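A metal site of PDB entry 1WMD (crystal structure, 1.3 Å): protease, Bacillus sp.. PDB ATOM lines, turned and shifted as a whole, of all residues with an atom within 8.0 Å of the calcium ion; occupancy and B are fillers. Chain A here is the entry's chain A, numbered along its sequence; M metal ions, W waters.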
ATOM      1  N   LEU A 349      15.509   4.702 -35.266  1.00  0.00           N
ATOM      2  CA  LEU A 349      15.951   5.104 -33.935  1.00  0.00           C
ATOM      3  C   LEU A 349      17.472   5.153 -33.959  1.00  0.00           C
ATOM      4  O   LEU A 349      18.159   4.176 -34.329  1.00  0.00           O
ATOM      5  CB  LEU A 349      15.480   4.075 -32.915  1.00  0.00           C
ATOM      6  CG  LEU A 349      16.146   4.145 -31.545  1.00  0.00           C
ATOM      7  CD1 LEU A 349      15.679   5.377 -30.818  1.00  0.00           C
ATOM      8  CD2 LEU A 349      15.784   2.872 -30.764  1.00  0.00           C
ATOM      9  N   TRP A 351      21.025   6.686 -31.676  1.00  0.00           N
ATOM     10  CA  TRP A 351      21.548   7.379 -30.491  1.00  0.00           C
ATOM     11  C   TRP A 351      23.056   7.591 -30.635  1.00  0.00           C
ATOM     12  O   TRP A 351      23.729   6.783 -31.278  1.00  0.00           O
ATOM     13  CB  TRP A 351      21.226   6.670 -29.191  1.00  0.00           C
ATOM     14  CG  TRP A 351      21.576   5.238 -28.939  1.00  0.00           C
ATOM     15  CD1 TRP A 351      22.573   4.776 -28.140  1.00  0.00           C
ATOM     16  CD2 TRP A 351      20.971   4.057 -29.482  1.00  0.00           C
ATOM     17  NE1 TRP A 351      22.637   3.408 -28.116  1.00  0.00           N
ATOM     18  CE2 TRP A 351      21.651   2.929 -28.931  1.00  0.00           C
ATOM     19  CE3 TRP A 351      19.911   3.780 -30.339  1.00  0.00           C
ATOM     20  CZ2 TRP A 351      21.328   1.611 -29.227  1.00  0.00           C
ATOM     21  CZ3 TRP A 351      19.569   2.497 -30.650  1.00  0.00           C
ATOM     22  CH2 TRP A 351      20.280   1.398 -30.096  1.00  0.00           C
ATOM     23  N   LEU A 364      29.000  -1.558 -28.577  1.00  0.00           N
ATOM     24  CA  LEU A 364      27.790  -0.902 -28.038  1.00  0.00           C
ATOM     25  C   LEU A 364      27.857  -0.850 -26.524  1.00  0.00           C
ATOM     26  O   LEU A 364      28.208  -1.845 -25.849  1.00  0.00           O
ATOM     27  CB  LEU A 364      26.526  -1.634 -28.490  1.00  0.00           C
ATOM     28  CG  LEU A 364      25.210  -0.900 -28.222  1.00  0.00           C
ATOM     29  CD1 LEU A 364      25.050   0.314 -29.129  1.00  0.00           C
ATOM     30  CD2 LEU A 364      24.062  -1.902 -28.388  1.00  0.00           C
ATOM     31  N   ASN A 366      25.459   1.448 -24.501  1.00  0.00           N
ATOM     32  CA  ASN A 366      24.039   1.539 -24.084  1.00  0.00           C
ATOM     33  C   ASN A 366      23.135   0.945 -25.161  1.00  0.00           C
ATOM     34  O   ASN A 366      23.244   1.344 -26.342  1.00  0.00           O
ATOM     35  CB  ASN A 366      23.646   2.985 -23.812  1.00  0.00           C
ATOM     36  CG  ASN A 366      24.434   3.612 -22.669  1.00  0.00           C
ATOM     37  OD1 ASN A 366      24.727   2.913 -21.665  1.00  0.00           O
ATOM     38  ND2 ASN A 366      24.695   4.906 -22.787  1.00  0.00           N
ATOM     39  N   ASP A 367      22.312  -0.021 -24.771  1.00  0.00           N
ATOM     40  CA  ASP A 367      21.473  -0.754 -25.696  1.00  0.00           C
ATOM     41  C   ASP A 367      20.003  -0.362 -25.540  1.00  0.00           C
ATOM     42  O   ASP A 367      19.371  -0.700 -24.559  1.00  0.00           O
ATOM     43  CB  ASP A 367      21.637  -2.236 -25.430  1.00  0.00           C
ATOM     44  CG  ASP A 367      20.868  -3.125 -26.369  1.00  0.00           C
ATOM     45  OD1 ASP A 367      20.255  -2.596 -27.315  1.00  0.00           O
ATOM     46  OD2 ASP A 367      20.882  -4.374 -26.171  1.00  0.00           O
ATOM     47  N   LEU A 368      19.520   0.395 -26.521  1.00  0.00           N
ATOM     48  CA  LEU A 368      18.086   0.690 -26.651  1.00  0.00           C
ATOM     49  C   LEU A 368      17.487  -0.242 -27.695  1.00  0.00           C
ATOM     50  O   LEU A 368      18.188  -0.643 -28.638  1.00  0.00           O
ATOM     51  CB  LEU A 368      17.905   2.129 -27.140  1.00  0.00           C
ATOM     52  CG  LEU A 368      18.589   3.228 -26.327  1.00  0.00           C
ATOM     53  CD1 LEU A 368      18.270   4.610 -26.896  1.00  0.00           C
ATOM     54  CD2 LEU A 368      18.175   3.163 -24.856  1.00  0.00           C
ATOM     55  N   ASP A 369      16.216  -0.599 -27.498  1.00  0.00           N
ATOM     56  CA  ASP A 369      15.482  -1.388 -28.478  1.00  0.00           C
ATOM     57  C   ASP A 369      14.253  -0.638 -29.012  1.00  0.00           C
ATOM     58  O   ASP A 369      13.524  -0.013 -28.235  1.00  0.00           O
ATOM     59  CB  ASP A 369      14.999  -2.709 -27.851  1.00  0.00           C
ATOM     60  CG  ASP A 369      16.128  -3.642 -27.451  1.00  0.00           C
ATOM     61  OD1 ASP A 369      17.226  -3.652 -28.131  1.00  0.00           O
ATOM     62  OD2 ASP A 369      15.970  -4.417 -26.481  1.00  0.00           O
ATOM     63  N   LEU A 370      13.995  -0.727 -30.304  1.00  0.00           N
ATOM     64  CA  LEU A 370      12.808  -0.124 -30.913  1.00  0.00           C
ATOM     65  C   LEU A 370      11.722  -1.168 -31.035  1.00  0.00           C
ATOM     66  O   LEU A 370      11.956  -2.266 -31.574  1.00  0.00           O
ATOM     67  CB  LEU A 370      13.235   0.405 -32.296  1.00  0.00           C
ATOM     68  CG  LEU A 370      12.070   1.066 -33.090  1.00  0.00           C
ATOM     69  CD1 LEU A 370      11.549   2.335 -32.410  1.00  0.00           C
ATOM     70  CD2 LEU A 370      12.537   1.361 -34.503  1.00  0.00           C
ATOM     71  N   VAL A 381      10.299  -5.550 -34.064  1.00  0.00           N
ATOM     72  CA  VAL A 381      11.473  -5.202 -33.287  1.00  0.00           C
ATOM     73  C   VAL A 381      12.528  -4.611 -34.211  1.00  0.00           C
ATOM     74  O   VAL A 381      12.653  -5.023 -35.376  1.00  0.00           O
ATOM     75  CB  VAL A 381      11.919  -6.483 -32.570  1.00  0.00           C
ATOM     76  CG1 VAL A 381      13.311  -6.439 -31.999  1.00  0.00           C
ATOM     77  CG2 VAL A 381      10.840  -6.709 -31.484  1.00  0.00           C
ATOM     78  N   GLY A 382      13.253  -3.625 -33.715  1.00  0.00           N
ATOM     79  CA  GLY A 382      14.200  -2.920 -34.588  1.00  0.00           C
ATOM     80  C   GLY A 382      15.171  -3.878 -35.238  1.00  0.00           C
ATOM     81  O   GLY A 382      15.735  -4.732 -34.556  1.00  0.00           O
ATOM     82  N   ASN A 383      15.365  -3.705 -36.547  1.00  0.00           N
ATOM     83  CA  ASN A 383      16.309  -4.438 -37.395  1.00  0.00           C
ATOM     84  C   ASN A 383      15.960  -5.929 -37.599  1.00  0.00           C
ATOM     85  O   ASN A 383      16.803  -6.660 -38.175  1.00  0.00           O
ATOM     86  CB  ASN A 383      17.753  -4.327 -36.938  1.00  0.00           C
ATOM     87  CG  ASN A 383      18.260  -2.886 -37.001  1.00  0.00           C
ATOM     88  OD1 ASN A 383      17.675  -2.070 -37.713  1.00  0.00           O
ATOM     89  ND2 ASN A 383      19.353  -2.591 -36.293  1.00  0.00           N
ATOM     90  N   TRP A 393      16.219  -9.782 -31.775  1.00  0.00           N
ATOM     91  CA  TRP A 393      16.577  -8.523 -31.129  1.00  0.00           C
ATOM     92  C   TRP A 393      18.017  -8.092 -31.361  1.00  0.00           C
ATOM     93  O   TRP A 393      18.945  -8.914 -31.459  1.00  0.00           O
ATOM     94  CB  TRP A 393      16.388  -8.660 -29.623  1.00  0.00           C
ATOM     95  CG  TRP A 393      14.983  -8.961 -29.236  1.00  0.00           C
ATOM     96  CD1 TRP A 393      14.349 -10.152 -29.313  1.00  0.00           C
ATOM     97  CD2 TRP A 393      14.055  -8.012 -28.693  1.00  0.00           C
ATOM     98  NE1 TRP A 393      13.062 -10.006 -28.861  1.00  0.00           N
ATOM     99  CE2 TRP A 393      12.852  -8.708 -28.468  1.00  0.00           C
ATOM    100  CE3 TRP A 393      14.112  -6.651 -28.389  1.00  0.00           C
ATOM    101  CZ2 TRP A 393      11.739  -8.027 -27.942  1.00  0.00           C
ATOM    102  CZ3 TRP A 393      13.018  -5.997 -27.867  1.00  0.00           C
ATOM    103  CH2 TRP A 393      11.818  -6.710 -27.639  1.00  0.00           C
ATOM    104  N   ASP A 394      18.172  -6.770 -31.450  1.00  0.00           N
ATOM    105  CA  ASP A 394      19.474  -6.201 -31.799  1.00  0.00           C
ATOM    106  C   ASP A 394      20.203  -5.781 -30.524  1.00  0.00           C
ATOM    107  O   ASP A 394      19.623  -4.964 -29.768  1.00  0.00           O
ATOM    108  CB  ASP A 394      19.277  -5.054 -32.760  1.00  0.00           C
ATOM    109  CG  ASP A 394      20.596  -4.552 -33.368  1.00  0.00           C
ATOM    110  OD1 ASP A 394      21.474  -4.158 -32.570  1.00  0.00           O
ATOM    111  OD2 ASP A 394      20.730  -4.518 -34.599  1.00  0.00           O
ATOM    112  N   GLY A 395      21.425  -6.253 -30.331  1.00  0.00           N
ATOM    113  CA  GLY A 395      22.293  -5.886 -29.232  1.00  0.00           C
ATOM    114  C   GLY A 395      23.627  -5.355 -29.669  1.00  0.00           C
ATOM    115  O   GLY A 395      24.602  -5.373 -28.880  1.00  0.00           O
ATOM    116  N   ARG A 396      23.719  -4.923 -30.922  1.00  0.00           N
ATOM    117  CA  ARG A 396      25.014  -4.447 -31.407  1.00  0.00           C
ATOM    118  C   ARG A 396      25.005  -3.063 -32.008  1.00  0.00           C
ATOM    119  O   ARG A 396      26.003  -2.307 -31.906  1.00  0.00           O
ATOM    120  CB  ARG A 396      25.495  -5.427 -32.511  1.00  0.00           C
ATOM    121  CG  ARG A 396      26.004  -6.726 -31.861  1.00  0.00           C
ATOM    122  CD  ARG A 396      27.244  -6.496 -31.001  1.00  0.00           C
ATOM    123  NE  ARG A 396      27.720  -7.747 -30.427  1.00  0.00           N
ATOM    124  CZ  ARG A 396      27.251  -8.361 -29.365  1.00  0.00           C
ATOM    125  NH1 ARG A 396      26.223  -7.854 -28.673  1.00  0.00           N
ATOM    126  NH2 ARG A 396      27.843  -9.503 -29.008  1.00  0.00           N
ATOM    127  N   ASN A 397      23.875  -2.709 -32.645  1.00  0.00           N
ATOM    128  CA  ASN A 397      23.812  -1.445 -33.361  1.00  0.00           C
ATOM    129  C   ASN A 397      23.211  -0.298 -32.549  1.00  0.00           C
ATOM    130  O   ASN A 397      22.329  -0.544 -31.748  1.00  0.00           O
ATOM    131  CB  ASN A 397      22.949  -1.672 -34.590  1.00  0.00           C
ATOM    132  CG  ASN A 397      23.630  -2.545 -35.624  1.00  0.00           C
ATOM    133  OD1 ASN A 397      24.660  -2.134 -36.190  1.00  0.00           O
ATOM    134  ND2 ASN A 397      23.089  -3.735 -35.827  1.00  0.00           N
ATOM    135  N   ASN A 398      23.654   0.945 -32.833  1.00  0.00           N
ATOM    136  CA  ASN A 398      23.035   2.139 -32.232  1.00  0.00           C
ATOM    137  C   ASN A 398      22.159   2.859 -33.286  1.00  0.00           C
ATOM    138  O   ASN A 398      21.889   4.044 -33.183  1.00  0.00           O
ATOM    139  CB  ASN A 398      24.080   3.067 -31.629  1.00  0.00           C
ATOM    140  CG  ASN A 398      25.169   3.533 -32.550  1.00  0.00           C
ATOM    141  OD1 ASN A 398      25.776   2.698 -33.227  1.00  0.00           O
ATOM    142  ND2 ASN A 398      25.447   4.829 -32.588  1.00  0.00           N
ATOM    143  N   VAL A 399      21.725   2.094 -34.297  1.00  0.00           N
ATOM    144  CA  VAL A 399      20.686   2.428 -35.271  1.00  0.00           C
ATOM    145  C   VAL A 399      19.718   1.241 -35.290  1.00  0.00           C
ATOM    146  O   VAL A 399      20.220   0.125 -35.522  1.00  0.00           O
ATOM    147  CB  VAL A 399      21.285   2.619 -36.685  1.00  0.00           C
ATOM    148  CG1 VAL A 399      20.150   2.965 -37.639  1.00  0.00           C
ATOM    149  CG2 VAL A 399      22.346   3.715 -36.659  1.00  0.00           C
ATOM    150  N   GLU A 400      18.459   1.494 -35.020  1.00  0.00           N
ATOM    151  CA  GLU A 400      17.461   0.392 -35.140  1.00  0.00           C
ATOM    152  C   GLU A 400      16.318   0.852 -36.037  1.00  0.00           C
ATOM    153  O   GLU A 400      15.935   2.023 -35.915  1.00  0.00           O
ATOM    154  CB  GLU A 400      16.923  -0.032 -33.768  1.00  0.00           C
ATOM    155  CG  GLU A 400      17.860  -0.981 -33.045  1.00  0.00           C
ATOM    156  CD  GLU A 400      17.185  -1.828 -31.983  1.00  0.00           C
ATOM    157  OE1 GLU A 400      15.922  -1.879 -31.956  1.00  0.00           O
ATOM    158  OE2 GLU A 400      17.918  -2.474 -31.189  1.00  0.00           O
ATOM    159  N   GLN A 417      12.828   1.279 -25.835  1.00  0.00           N
ATOM    160  CA  GLN A 417      13.012   0.564 -24.588  1.00  0.00           C
ATOM    161  C   GLN A 417      14.473   0.548 -24.207  1.00  0.00           C
ATOM    162  O   GLN A 417      15.352   0.201 -25.016  1.00  0.00           O
ATOM    163  CB  GLN A 417      12.494  -0.860 -24.797  1.00  0.00           C
ATOM    164  CG  GLN A 417      11.053  -0.897 -25.273  1.00  0.00           C
ATOM    165  CD  GLN A 417      10.524  -2.315 -25.277  1.00  0.00           C
ATOM    166  OE1 GLN A 417      11.272  -3.300 -25.249  1.00  0.00           O
ATOM    167  NE2 GLN A 417       9.202  -2.417 -25.330  1.00  0.00           N
ATOM    168  N   ALA A 418      14.737   0.913 -22.933  1.00  0.00           N
ATOM    169  CA  ALA A 418      16.148   0.880 -22.491  1.00  0.00           C
ATOM    170  C   ALA A 418      16.538  -0.512 -22.018  1.00  0.00           C
ATOM    171  O   ALA A 418      16.366  -0.873 -20.839  1.00  0.00           O
ATOM    172  CB  ALA A 418      16.370   1.913 -21.405  1.00  0.00           C
ATOM    173  N   TYR A 419      17.060  -1.387 -22.869  1.00  0.00           N
ATOM    174  CA  TYR A 419      17.393  -2.761 -22.453  1.00  0.00           C
ATOM    175  C   TYR A 419      18.538  -2.789 -21.440  1.00  0.00           C
ATOM    176  O   TYR A 419      18.468  -3.508 -20.422  1.00  0.00           O
ATOM    177  CB  TYR A 419      17.716  -3.616 -23.702  1.00  0.00           C
ATOM    178  CG  TYR A 419      18.089  -5.011 -23.309  1.00  0.00           C
ATOM    179  CD1 TYR A 419      17.116  -5.875 -22.828  1.00  0.00           C
ATOM    180  CD2 TYR A 419      19.411  -5.476 -23.407  1.00  0.00           C
ATOM    181  CE1 TYR A 419      17.442  -7.160 -22.445  1.00  0.00           C
ATOM    182  CE2 TYR A 419      19.768  -6.774 -23.020  1.00  0.00           C
ATOM    183  CZ  TYR A 419      18.758  -7.583 -22.567  1.00  0.00           C
ATOM    184  OH  TYR A 419      19.031  -8.849 -22.161  1.00  0.00           O
ATOM    185  N   ASN A 420      19.586  -2.023 -21.670  1.00  0.00           N
ATOM    186  CA  ASN A 420      20.740  -2.073 -20.769  1.00  0.00           C
ATOM    187  C   ASN A 420      21.549  -0.806 -20.996  1.00  0.00           C
ATOM    188  O   ASN A 420      22.144  -0.652 -22.069  1.00  0.00           O
ATOM    189  CB  ASN A 420      21.580  -3.313 -21.041  1.00  0.00           C
ATOM    190  CG  ASN A 420      22.670  -3.495 -20.014  1.00  0.00           C
ATOM    191  OD1 ASN A 420      22.826  -2.771 -19.026  1.00  0.00           O
ATOM    192  ND2 ASN A 420      23.491  -4.505 -20.225  1.00  0.00           N
HETATM  193 CA    CA M   1      19.010  -2.775 -29.236  1.00  0.00          CA
HETATM  194  O   HOH W   1      21.018  -2.451 -30.438  1.00  0.00           O
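N of Leu 370 lies within hydrogen-bond range of OE1 of Glu 400. The backbone carbonyl oxygen of Leu 349 lies within hydrogen-bond range of the backbone NH of Glu 400 (2.8 Å). The backbone NH of Asp 369 is in hydrogen-bond range of the backbone carbonyl oxygen of Gln 417 (2.7 Å). N of Tyr 419 is in hydrogen-bond range of O of Asp 367, 2.9 Å away. The backbone NH of Asp 367 sits at hydrogen-bond distance from the backbone carbonyl oxygen of Asn 420, at 2.8 Å. The side-chain amide nitrogen (ND2) of Asn 397 sits at hydrogen-bond distance from the side-chain carboxylate (OD2) of Asp 394 (2.8 Å). The backbone NH of Arg 396 sits at hydrogen-bond distance from the side-chain carboxylate of Asp 394 (2.9 Å). ND2 of Asn 383 sits at hydrogen-bond distance from OD2 of Asp 394 (2.9 Å).
Within 4 Å of the calcium ion: Asp 367, Leu 368, Asp 369, Asp 394 and Glu 400.
The side-chain carboxylate (OE2) of Glu 400 is bound to the calcium ion. The calcium ion is bound by the side-chain carboxylate (OD1) of Asp 369 (2.3 Å). OD1 of Asp 367 binds the calcium ion, at 2.3 Å. The calcium ion is bound by O of Asp 394 (2.3 Å). The backbone carbonyl oxygen (O) of Leu 368 is bound to the calcium ion (2.4 Å). Water W1 is bound to the calcium ion (2.4 Å). The calcium ion has six donor atoms within binding distance.
Water W1 lies within hydrogen-bond range of O of Asn 397 (2.7 Å) and OD1 of Asp 394 (2.8 Å).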
